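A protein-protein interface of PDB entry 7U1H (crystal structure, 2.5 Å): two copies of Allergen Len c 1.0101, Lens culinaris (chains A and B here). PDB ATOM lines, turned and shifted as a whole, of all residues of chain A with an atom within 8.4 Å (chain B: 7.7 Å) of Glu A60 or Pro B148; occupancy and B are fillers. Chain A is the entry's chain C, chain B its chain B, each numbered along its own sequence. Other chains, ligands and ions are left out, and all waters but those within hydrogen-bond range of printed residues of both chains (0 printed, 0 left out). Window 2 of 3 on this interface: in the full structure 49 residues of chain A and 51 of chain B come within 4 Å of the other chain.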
ATOM      1  N   ARG A  51     -15.989   5.409 -25.982  1.00  0.00           N
ATOM      2  CA  ARG A  51     -16.753   5.758 -24.755  1.00  0.00           C
ATOM      3  C   ARG A  51     -15.773   5.845 -23.585  1.00  0.00           C
ATOM      4  O   ARG A  51     -14.882   4.996 -23.480  1.00  0.00           O
ATOM      5  CB  ARG A  51     -17.846   4.727 -24.475  1.00  0.00           C
ATOM      6  CG  ARG A  51     -19.045   4.840 -25.404  1.00  0.00           C
ATOM      7  CD  ARG A  51     -19.935   3.611 -25.415  1.00  0.00           C
ATOM      8  NE  ARG A  51     -20.397   3.254 -24.079  1.00  0.00           N
ATOM      9  CZ  ARG A  51     -21.663   3.205 -23.679  1.00  0.00           C
ATOM     10  NH1 ARG A  51     -22.642   3.491 -24.528  1.00  0.00           N
ATOM     11  NH2 ARG A  51     -21.933   2.855 -22.425  1.00  0.00           N
ATOM     12  N   PHE A  52     -15.904   6.880 -22.767  1.00  0.00           N
ATOM     13  CA  PHE A  52     -15.027   7.122 -21.598  1.00  0.00           C
ATOM     14  C   PHE A  52     -15.130   5.939 -20.620  1.00  0.00           C
ATOM     15  O   PHE A  52     -14.079   5.510 -20.103  1.00  0.00           O
ATOM     16  CB  PHE A  52     -15.392   8.442 -20.920  1.00  0.00           C
ATOM     17  CG  PHE A  52     -15.042   9.687 -21.688  1.00  0.00           C
ATOM     18  CD1 PHE A  52     -13.717  10.012 -21.938  1.00  0.00           C
ATOM     19  CD2 PHE A  52     -16.033  10.545 -22.125  1.00  0.00           C
ATOM     20  CE1 PHE A  52     -13.388  11.160 -22.629  1.00  0.00           C
ATOM     21  CE2 PHE A  52     -15.701  11.696 -22.820  1.00  0.00           C
ATOM     22  CZ  PHE A  52     -14.379  12.010 -23.051  1.00  0.00           C
ATOM     23  N   ASP A  53     -16.340   5.415 -20.389  1.00  0.00           N
ATOM     24  CA  ASP A  53     -16.596   4.343 -19.382  1.00  0.00           C
ATOM     25  C   ASP A  53     -16.042   2.991 -19.863  1.00  0.00           C
ATOM     26  O   ASP A  53     -15.827   2.153 -18.974  1.00  0.00           O
ATOM     27  CB  ASP A  53     -18.073   4.247 -18.989  1.00  0.00           C
ATOM     28  CG  ASP A  53     -19.009   4.134 -20.177  1.00  0.00           C
ATOM     29  OD1 ASP A  53     -18.988   5.035 -21.038  1.00  0.00           O
ATOM     30  OD2 ASP A  53     -19.747   3.153 -20.230  1.00  0.00           O
ATOM     31  N   LYS A  54     -15.794   2.797 -21.173  1.00  0.00           N
ATOM     32  CA  LYS A  54     -15.135   1.582 -21.753  1.00  0.00           C
ATOM     33  C   LYS A  54     -13.619   1.640 -21.560  1.00  0.00           C
ATOM     34  O   LYS A  54     -13.029   0.581 -21.331  1.00  0.00           O
ATOM     35  CB  LYS A  54     -15.424   1.396 -23.245  1.00  0.00           C
ATOM     36  CG  LYS A  54     -16.829   0.913 -23.601  1.00  0.00           C
ATOM     37  CD  LYS A  54     -17.639   0.297 -22.452  1.00  0.00           C
ATOM     38  CE  LYS A  54     -19.107   0.057 -22.773  1.00  0.00           C
ATOM     39  NZ  LYS A  54     -19.462  -1.386 -22.864  1.00  0.00           N
ATOM     40  N   SER A  56     -12.238   3.028 -18.977  1.00  0.00           N
ATOM     41  CA  SER A  56     -12.121   2.721 -17.530  1.00  0.00           C
ATOM     42  C   SER A  56     -13.417   3.007 -16.774  1.00  0.00           C
ATOM     43  O   SER A  56     -13.919   4.126 -16.890  1.00  0.00           O
ATOM     44  CB  SER A  56     -11.017   3.500 -16.901  1.00  0.00           C
ATOM     45  OG  SER A  56     -11.183   3.499 -15.491  1.00  0.00           O
ATOM     46  N   LYS A  57     -13.845   2.053 -15.941  1.00  0.00           N
ATOM     47  CA  LYS A  57     -14.904   2.200 -14.912  1.00  0.00           C
ATOM     48  C   LYS A  57     -14.671   3.490 -14.111  1.00  0.00           C
ATOM     49  O   LYS A  57     -15.640   4.029 -13.579  1.00  0.00           O
ATOM     50  CB  LYS A  57     -14.935   0.945 -14.026  1.00  0.00           C
ATOM     51  CG  LYS A  57     -15.596  -0.274 -14.664  1.00  0.00           C
ATOM     52  CD  LYS A  57     -14.733  -1.543 -14.712  1.00  0.00           C
ATOM     53  CE  LYS A  57     -15.175  -2.505 -15.805  1.00  0.00           C
ATOM     54  NZ  LYS A  57     -14.688  -3.892 -15.584  1.00  0.00           N
ATOM     55  N   ILE A  58     -13.433   3.968 -14.004  1.00  0.00           N
ATOM     56  CA  ILE A  58     -13.091   5.244 -13.308  1.00  0.00           C
ATOM     57  C   ILE A  58     -13.979   6.372 -13.849  1.00  0.00           C
ATOM     58  O   ILE A  58     -14.293   7.289 -13.086  1.00  0.00           O
ATOM     59  CB  ILE A  58     -11.580   5.528 -13.448  1.00  0.00           C
ATOM     60  CG1 ILE A  58     -10.818   5.035 -12.215  1.00  0.00           C
ATOM     61  CG2 ILE A  58     -11.266   6.989 -13.765  1.00  0.00           C
ATOM     62  CD1 ILE A  58     -10.741   3.527 -12.107  1.00  0.00           C
ATOM     63  N   PHE A  59     -14.391   6.296 -15.117  1.00  0.00           N
ATOM     64  CA  PHE A  59     -15.186   7.346 -15.795  1.00  0.00           C
ATOM     65  C   PHE A  59     -16.683   6.993 -15.844  1.00  0.00           C
ATOM     66  O   PHE A  59     -17.341   7.526 -16.736  1.00  0.00           O
ATOM     67  CB  PHE A  59     -14.617   7.572 -17.196  1.00  0.00           C
ATOM     68  CG  PHE A  59     -13.169   7.988 -17.223  1.00  0.00           C
ATOM     69  CD1 PHE A  59     -12.740   9.103 -16.534  1.00  0.00           C
ATOM     70  CD2 PHE A  59     -12.243   7.273 -17.956  1.00  0.00           C
ATOM     71  CE1 PHE A  59     -11.406   9.472 -16.561  1.00  0.00           C
ATOM     72  CE2 PHE A  59     -10.912   7.640 -17.977  1.00  0.00           C
ATOM     73  CZ  PHE A  59     -10.495   8.735 -17.277  1.00  0.00           C
ATOM     74  N   GLU A  60     -17.210   6.208 -14.888  1.00  0.00           N
ATOM     75  CA  GLU A  60     -18.644   5.797 -14.823  1.00  0.00           C
ATOM     76  C   GLU A  60     -19.554   7.005 -15.106  1.00  0.00           C
ATOM     77  O   GLU A  60     -20.525   6.821 -15.862  1.00  0.00           O
ATOM     78  CB  GLU A  60     -18.968   5.199 -13.451  1.00  0.00           C
ATOM     79  CG  GLU A  60     -20.043   4.128 -13.487  1.00  0.00           C
ATOM     80  CD  GLU A  60     -21.379   4.496 -12.865  1.00  0.00           C
ATOM     81  OE1 GLU A  60     -21.607   5.690 -12.593  1.00  0.00           O
ATOM     82  OE2 GLU A  60     -22.182   3.577 -12.654  1.00  0.00           O
ATOM     83  N   ASN A  61     -19.247   8.160 -14.505  1.00  0.00           N
ATOM     84  CA  ASN A  61     -20.132   9.351 -14.494  1.00  0.00           C
ATOM     85  C   ASN A  61     -20.085  10.060 -15.838  1.00  0.00           C
ATOM     86  O   ASN A  61     -20.911  10.953 -16.053  1.00  0.00           O
ATOM     87  CB  ASN A  61     -19.703  10.363 -13.434  1.00  0.00           C
ATOM     88  CG  ASN A  61     -20.258  10.060 -12.065  1.00  0.00           C
ATOM     89  OD1 ASN A  61     -20.590   8.922 -11.752  1.00  0.00           O
ATOM     90  ND2 ASN A  61     -20.366  11.090 -11.250  1.00  0.00           N
ATOM     91  N   LEU A  62     -19.094   9.739 -16.666  1.00  0.00           N
ATOM     92  CA  LEU A  62     -18.964  10.310 -18.029  1.00  0.00           C
ATOM     93  C   LEU A  62     -19.587   9.374 -19.069  1.00  0.00           C
ATOM     94  O   LEU A  62     -19.426   9.706 -20.246  1.00  0.00           O
ATOM     95  CB  LEU A  62     -17.485  10.559 -18.371  1.00  0.00           C
ATOM     96  CG  LEU A  62     -16.778  11.750 -17.721  1.00  0.00           C
ATOM     97  CD1 LEU A  62     -15.425  11.933 -18.386  1.00  0.00           C
ATOM     98  CD2 LEU A  62     -17.597  13.043 -17.776  1.00  0.00           C
ATOM     99  N   GLN A  63     -20.284   8.300 -18.656  1.00  0.00           N
ATOM    100  CA  GLN A  63     -20.795   7.212 -19.543  1.00  0.00           C
ATOM    101  C   GLN A  63     -21.728   7.824 -20.597  1.00  0.00           C
ATOM    102  O   GLN A  63     -21.767   7.258 -21.699  1.00  0.00           O
ATOM    103  CB  GLN A  63     -21.426   6.059 -18.747  1.00  0.00           C
ATOM    104  CG  GLN A  63     -22.950   5.958 -18.819  1.00  0.00           C
ATOM    105  CD  GLN A  63     -23.641   5.717 -17.492  1.00  0.00           C
ATOM    106  OE1 GLN A  63     -24.620   4.972 -17.397  1.00  0.00           O
ATOM    107  NE2 GLN A  63     -23.161   6.378 -16.448  1.00  0.00           N
ATOM    108  N   ASN A  64     -22.384   8.958 -20.287  1.00  0.00           N
ATOM    109  CA  ASN A  64     -23.344   9.648 -21.192  1.00  0.00           C
ATOM    110  C   ASN A  64     -22.737  10.916 -21.809  1.00  0.00           C
ATOM    111  O   ASN A  64     -23.486  11.873 -22.024  1.00  0.00           O
ATOM    112  CB  ASN A  64     -24.684   9.987 -20.522  1.00  0.00           C
ATOM    113  CG  ASN A  64     -25.780  10.197 -21.554  1.00  0.00           C
ATOM    114  OD1 ASN A  64     -25.888   9.429 -22.511  1.00  0.00           O
ATOM    115  ND2 ASN A  64     -26.554  11.266 -21.422  1.00  0.00           N
ATOM    116  N   TYR A  65     -21.444  10.932 -22.129  1.00  0.00           N
ATOM    117  CA  TYR A  65     -20.803  12.024 -22.904  1.00  0.00           C
ATOM    118  C   TYR A  65     -19.946  11.406 -24.007  1.00  0.00           C
ATOM    119  O   TYR A  65     -19.221  10.454 -23.730  1.00  0.00           O
ATOM    120  CB  TYR A  65     -20.005  12.926 -21.976  1.00  0.00           C
ATOM    121  CG  TYR A  65     -20.869  13.675 -21.000  1.00  0.00           C
ATOM    122  CD1 TYR A  65     -21.425  14.886 -21.353  1.00  0.00           C
ATOM    123  CD2 TYR A  65     -21.148  13.174 -19.741  1.00  0.00           C
ATOM    124  CE1 TYR A  65     -22.233  15.590 -20.482  1.00  0.00           C
ATOM    125  CE2 TYR A  65     -21.971  13.857 -18.864  1.00  0.00           C
ATOM    126  CZ  TYR A  65     -22.493  15.085 -19.228  1.00  0.00           C
ATOM    127  OH  TYR A  65     -23.285  15.824 -18.396  1.00  0.00           O
ATOM    128  N   PRO A 148     -27.700   5.631 -22.234  1.00  0.00           N
ATOM    129  CA  PRO A 148     -26.379   6.083 -21.822  1.00  0.00           C
ATOM    130  C   PRO A 148     -25.330   5.820 -22.914  1.00  0.00           C
ATOM    131  O   PRO A 148     -25.005   4.676 -23.158  1.00  0.00           O
ATOM    132  CB  PRO A 148     -26.206   5.300 -20.516  1.00  0.00           C
ATOM    133  CG  PRO A 148     -27.589   5.355 -19.930  1.00  0.00           C
ATOM    134  CD  PRO A 148     -28.448   5.022 -21.130  1.00  0.00           C
ATOM    135  N   ILE A 300     -15.731  18.194 -13.941  1.00  0.00           N
ATOM    136  CA  ILE A 300     -14.923  17.186 -14.672  1.00  0.00           C
ATOM    137  C   ILE A 300     -14.685  17.715 -16.086  1.00  0.00           C
ATOM    138  O   ILE A 300     -15.670  17.958 -16.814  1.00  0.00           O
ATOM    139  CB  ILE A 300     -15.653  15.834 -14.679  1.00  0.00           C
ATOM    140  CG1 ILE A 300     -15.854  15.318 -13.260  1.00  0.00           C
ATOM    141  CG2 ILE A 300     -14.921  14.817 -15.551  1.00  0.00           C
ATOM    142  CD1 ILE A 300     -16.968  14.328 -13.121  1.00  0.00           C
ATOM    143  N   ARG B  51     -20.695   1.716   2.540  1.00  0.00           N
ATOM    144  CA  ARG B  51     -21.609   2.076   1.433  1.00  0.00           C
ATOM    145  C   ARG B  51     -22.977   1.478   1.755  1.00  0.00           C
ATOM    146  O   ARG B  51     -23.005   0.322   2.150  1.00  0.00           O
ATOM    147  CB  ARG B  51     -21.047   1.540   0.113  1.00  0.00           C
ATOM    148  CG  ARG B  51     -19.995   2.432  -0.530  1.00  0.00           C
ATOM    149  CD  ARG B  51     -20.594   3.309  -1.626  1.00  0.00           C
ATOM    150  NE  ARG B  51     -20.732   2.590  -2.889  1.00  0.00           N
ATOM    151  CZ  ARG B  51     -19.718   2.245  -3.685  1.00  0.00           C
ATOM    152  NH1 ARG B  51     -19.955   1.563  -4.796  1.00  0.00           N
ATOM    153  NH2 ARG B  51     -18.477   2.582  -3.375  1.00  0.00           N
ATOM    154  N   ASP B  53     -25.417   0.711  -0.313  1.00  0.00           N
ATOM    155  CA  ASP B  53     -25.701  -0.365  -1.305  1.00  0.00           C
ATOM    156  C   ASP B  53     -24.863  -1.621  -1.020  1.00  0.00           C
ATOM    157  O   ASP B  53     -25.341  -2.696  -1.350  1.00  0.00           O
ATOM    158  CB  ASP B  53     -25.584   0.101  -2.757  1.00  0.00           C
ATOM    159  CG  ASP B  53     -24.231   0.653  -3.139  1.00  0.00           C
ATOM    160  OD1 ASP B  53     -23.743   1.523  -2.405  1.00  0.00           O
ATOM    161  OD2 ASP B  53     -23.699   0.227  -4.185  1.00  0.00           O
ATOM    162  N   GLU B  60     -29.840   1.117  -3.297  1.00  0.00           N
ATOM    163  CA  GLU B  60     -29.031   1.512  -4.483  1.00  0.00           C
ATOM    164  C   GLU B  60     -29.244   3.006  -4.784  1.00  0.00           C
ATOM    165  O   GLU B  60     -28.311   3.629  -5.297  1.00  0.00           O
ATOM    166  CB  GLU B  60     -29.305   0.610  -5.679  1.00  0.00           C
ATOM    167  CG  GLU B  60     -30.514   1.002  -6.493  1.00  0.00           C
ATOM    168  CD  GLU B  60     -30.791  -0.034  -7.567  1.00  0.00           C
ATOM    169  OE1 GLU B  60     -31.500  -1.020  -7.264  1.00  0.00           O
ATOM    170  OE2 GLU B  60     -30.256   0.125  -8.685  1.00  0.00           O
ATOM    171  N   LEU B  62     -29.184   5.293  -2.668  1.00  0.00           N
ATOM    172  CA  LEU B  62     -28.350   6.015  -1.656  1.00  0.00           C
ATOM    173  C   LEU B  62     -26.845   5.769  -1.909  1.00  0.00           C
ATOM    174  O   LEU B  62     -26.028   6.243  -1.119  1.00  0.00           O
ATOM    175  CB  LEU B  62     -28.758   5.580  -0.236  1.00  0.00           C
ATOM    176  CG  LEU B  62     -30.041   6.195   0.353  1.00  0.00           C
ATOM    177  CD1 LEU B  62     -30.101   5.971   1.860  1.00  0.00           C
ATOM    178  CD2 LEU B  62     -30.185   7.689   0.050  1.00  0.00           C
ATOM    179  N   GLN B  63     -26.517   5.104  -3.017  1.00  0.00           N
ATOM    180  CA  GLN B  63     -25.165   4.706  -3.486  1.00  0.00           C
ATOM    181  C   GLN B  63     -24.186   5.888  -3.463  1.00  0.00           C
ATOM    182  O   GLN B  63     -23.014   5.651  -3.101  1.00  0.00           O
ATOM    183  CB  GLN B  63     -25.314   4.125  -4.895  1.00  0.00           C
ATOM    184  CG  GLN B  63     -24.087   4.263  -5.791  1.00  0.00           C
ATOM    185  CD  GLN B  63     -24.298   3.610  -7.137  1.00  0.00           C
ATOM    186  OE1 GLN B  63     -23.420   3.611  -7.995  1.00  0.00           O
ATOM    187  NE2 GLN B  63     -25.485   3.056  -7.334  1.00  0.00           N
ATOM    188  N   ASN B  64     -24.637   7.088  -3.850  1.00  0.00           N
ATOM    189  CA  ASN B  64     -23.786   8.305  -3.911  1.00  0.00           C
ATOM    190  C   ASN B  64     -23.950   9.155  -2.646  1.00  0.00           C
ATOM    191  O   ASN B  64     -23.771  10.370  -2.750  1.00  0.00           O
ATOM    192  CB  ASN B  64     -24.057   9.196  -5.131  1.00  0.00           C
ATOM    193  CG  ASN B  64     -22.908  10.160  -5.361  1.00  0.00           C
ATOM    194  OD1 ASN B  64     -21.754   9.725  -5.450  1.00  0.00           O
ATOM    195  ND2 ASN B  64     -23.192  11.459  -5.371  1.00  0.00           N
ATOM    196  N   TYR B  65     -24.246   8.534  -1.503  1.00  0.00           N
ATOM    197  CA  TYR B  65     -24.331   9.173  -0.173  1.00  0.00           C
ATOM    198  C   TYR B  65     -23.422   8.420   0.821  1.00  0.00           C
ATOM    199  O   TYR B  65     -23.662   7.237   1.133  1.00  0.00           O
ATOM    200  CB  TYR B  65     -25.800   9.249   0.242  1.00  0.00           C
ATOM    201  CG  TYR B  65     -26.608  10.144  -0.651  1.00  0.00           C
ATOM    202  CD1 TYR B  65     -26.594  11.514  -0.464  1.00  0.00           C
ATOM    203  CD2 TYR B  65     -27.363   9.631  -1.698  1.00  0.00           C
ATOM    204  CE1 TYR B  65     -27.304  12.357  -1.306  1.00  0.00           C
ATOM    205  CE2 TYR B  65     -28.073  10.458  -2.551  1.00  0.00           C
ATOM    206  CZ  TYR B  65     -28.036  11.827  -2.359  1.00  0.00           C
ATOM    207  OH  TYR B  65     -28.738  12.668  -3.172  1.00  0.00           O
ATOM    208  N   ARG B  66     -22.372   9.090   1.284  1.00  0.00           N
ATOM    209  CA  ARG B  66     -21.485   8.570   2.343  1.00  0.00           C
ATOM    210  C   ARG B  66     -21.717   9.385   3.627  1.00  0.00           C
ATOM    211  O   ARG B  66     -22.202  10.550   3.534  1.00  0.00           O
ATOM    212  CB  ARG B  66     -20.026   8.602   1.886  1.00  0.00           C
ATOM    213  CG  ARG B  66     -19.719   7.810   0.627  1.00  0.00           C
ATOM    214  CD  ARG B  66     -20.233   6.401   0.637  1.00  0.00           C
ATOM    215  NE  ARG B  66     -19.487   5.567   1.556  1.00  0.00           N
ATOM    216  CZ  ARG B  66     -18.301   5.004   1.321  1.00  0.00           C
ATOM    217  NH1 ARG B  66     -17.659   5.167   0.170  1.00  0.00           N
ATOM    218  NH2 ARG B  66     -17.752   4.270   2.272  1.00  0.00           N
ATOM    219  N   PRO B 144     -20.381  12.564  -3.219  1.00  0.00           N
ATOM    220  CA  PRO B 144     -19.362  12.520  -4.253  1.00  0.00           C
ATOM    221  C   PRO B 144     -19.792  13.106  -5.599  1.00  0.00           C
ATOM    222  O   PRO B 144     -20.918  12.990  -5.963  1.00  0.00           O
ATOM    223  CB  PRO B 144     -19.121  11.016  -4.356  1.00  0.00           C
ATOM    224  CG  PRO B 144     -19.207  10.551  -2.929  1.00  0.00           C
ATOM    225  CD  PRO B 144     -20.390  11.329  -2.415  1.00  0.00           C
ATOM    226  N   VAL B 145     -18.843  13.745  -6.283  1.00  0.00           N
ATOM    227  CA  VAL B 145     -19.053  14.345  -7.623  1.00  0.00           C
ATOM    228  C   VAL B 145     -18.341  13.514  -8.703  1.00  0.00           C
ATOM    229  O   VAL B 145     -18.854  13.502  -9.820  1.00  0.00           O
ATOM    230  CB  VAL B 145     -18.660  15.826  -7.618  1.00  0.00           C
ATOM    231  CG1 VAL B 145     -17.449  16.125  -6.771  1.00  0.00           C
ATOM    232  CG2 VAL B 145     -18.440  16.319  -9.018  1.00  0.00           C
ATOM    233  N   ASN B 146     -17.275  12.764  -8.401  1.00  0.00           N
ATOM    234  CA  ASN B 146     -16.483  12.071  -9.461  1.00  0.00           C
ATOM    235  C   ASN B 146     -17.143  10.725  -9.766  1.00  0.00           C
ATOM    236  O   ASN B 146     -17.856  10.687 -10.744  1.00  0.00           O
ATOM    237  CB  ASN B 146     -14.985  11.960  -9.147  1.00  0.00           C
ATOM    238  CG  ASN B 146     -14.226  13.236  -9.436  1.00  0.00           C
ATOM    239  OD1 ASN B 146     -14.332  13.795 -10.532  1.00  0.00           O
ATOM    240  ND2 ASN B 146     -13.434  13.692  -8.478  1.00  0.00           N
ATOM    241  N   ARG B 147     -16.895   9.669  -8.989  1.00  0.00           N
ATOM    242  CA  ARG B 147     -17.527   8.328  -9.154  1.00  0.00           C
ATOM    243  C   ARG B 147     -18.590   8.163  -8.083  1.00  0.00           C
ATOM    244  O   ARG B 147     -18.406   8.667  -6.977  1.00  0.00           O
ATOM    245  CB  ARG B 147     -16.556   7.166  -8.928  1.00  0.00           C
ATOM    246  CG  ARG B 147     -15.622   6.833 -10.084  1.00  0.00           C
ATOM    247  CD  ARG B 147     -14.220   6.601  -9.528  1.00  0.00           C
ATOM    248  NE  ARG B 147     -13.902   7.686  -8.611  1.00  0.00           N
ATOM    249  CZ  ARG B 147     -13.111   7.598  -7.561  1.00  0.00           C
ATOM    250  NH1 ARG B 147     -12.525   6.452  -7.270  1.00  0.00           N
ATOM    251  NH2 ARG B 147     -12.923   8.666  -6.808  1.00  0.00           N
ATOM    252  N   PRO B 148     -19.679   7.399  -8.355  1.00  0.00           N
ATOM    253  CA  PRO B 148     -20.753   7.225  -7.379  1.00  0.00           C
ATOM    254  C   PRO B 148     -20.199   6.610  -6.082  1.00  0.00           C
ATOM    255  O   PRO B 148     -19.660   5.504  -6.113  1.00  0.00           O
ATOM    256  CB  PRO B 148     -21.741   6.255  -8.033  1.00  0.00           C
ATOM    257  CG  PRO B 148     -21.323   6.169  -9.483  1.00  0.00           C
ATOM    258  CD  PRO B 148     -19.862   6.541  -9.533  1.00  0.00           C
ATOM    259  N   GLY B 149     -20.282   7.348  -4.982  1.00  0.00           N
ATOM    260  CA  GLY B 149     -20.009   6.794  -3.649  1.00  0.00           C
ATOM    261  C   GLY B 149     -18.538   6.806  -3.337  1.00  0.00           C
ATOM    262  O   GLY B 149     -18.208   6.415  -2.220  1.00  0.00           O
ATOM    263  N   GLN B 150     -17.692   7.278  -4.258  1.00  0.00           N
ATOM    264  CA  GLN B 150     -16.218   7.296  -4.081  1.00  0.00           C
ATOM    265  C   GLN B 150     -15.756   8.661  -3.557  1.00  0.00           C
ATOM    266  O   GLN B 150     -16.011   9.665  -4.231  1.00  0.00           O
ATOM    267  CB  GLN B 150     -15.488   6.959  -5.384  1.00  0.00           C
ATOM    268  CG  GLN B 150     -14.757   5.612  -5.362  1.00  0.00           C
ATOM    269  CD  GLN B 150     -15.409   4.542  -6.213  1.00  0.00           C
ATOM    270  OE1 GLN B 150     -14.749   3.866  -7.005  1.00  0.00           O
ATOM    271  NE2 GLN B 150     -16.719   4.380  -6.057  1.00  0.00           N
ATOM    272  N   LEU B 151     -15.072   8.657  -2.405  1.00  0.00           N
ATOM    273  CA  LEU B 151     -14.390   9.814  -1.753  1.00  0.00           C
ATOM    274  C   LEU B 151     -12.883   9.760  -2.077  1.00  0.00           C
ATOM    275  O   LEU B 151     -12.252   8.791  -1.668  1.00  0.00           O
ATOM    276  CB  LEU B 151     -14.608   9.738  -0.230  1.00  0.00           C
ATOM    277  CG  LEU B 151     -15.983  10.114   0.319  1.00  0.00           C
ATOM    278  CD1 LEU B 151     -16.394  11.521  -0.079  1.00  0.00           C
ATOM    279  CD2 LEU B 151     -17.036   9.148  -0.142  1.00  0.00           C
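ND2 of Asn A61 is in hydrogen-bond range of O of Val B145. O of Asn B146 is in hydrogen-bond range of ND2 of Asn A61.
Of the 16 printed residues of chain B, 4 touch a printed residue of chain A. Hydrophobic or aromatic side chains of chain B within 4 Å of the printed part of chain A: Pro B148. Among the printed residues, no Asp or Glu carboxylate lies within 4 Å of a Lys or Arg side-chain nitrogen of the other chain.
Glu A60 touches Pro B148, but with the chains exchanged Pro A148 does not touch Glu B60 (12.7 Å). Of the 7 pairs that touch across the chains among the printed residues, none has its exchanged pair printed and touching as well.
Printed residues of chain B within 4 Å of Glu A60: Pro B148 (3.2 Å). Printed residues of chain A within 4 Å of Pro B148: Glu A60 and Asn A61. No residue of chain A comes within 4 Å of Gly B149. Of the printed residues of chain A, Asn B146 touches Asn A61 and Ile A300. Of the printed residues of chain B, Asn A61 touches Val B145 (3.2 Å), Asn B146 (2.6 Å) and Pro B148 (3.3 Å). Of the printed residues of chain B, Ile A58 touches Arg B147. Tyr A65 touches none of the printed residues of chain B. Phe A52 touches none of the printed residues of chain B.
Ile A58 touches Arg B147. OE1 of Glu A60 touches CG of Pro B148, at 3.2 Å. Pro B148 touches Asn A61 (CD to OD1, 3.3 Å). Val B145 touches Ile A300 (O to CD1, 3.9 Å). OD1 of Asn B146 touches CG1 of Ile A300, 3.5 Å away.
The side-chain amide nitrogen (NE2) of Gln B150 lies within hydrogen-bond range of the backbone carbonyl oxygen (O) of Pro B148, at 3.1 Å. N of Ile A58 sits at hydrogen-bond distance from OG of Ser A56, at 2.7 Å. The side-chain amide oxygen (OD1) of Asn A61 lies close to the side-chain carboxylate (OE1) of Glu A60, at 3.5 Å. OE1 of Gln B150 lies close to NH1 of Arg B147. O of Glu A60 lies within hydrogen-bond range of NE2 of Gln A63 (2.7 Å).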
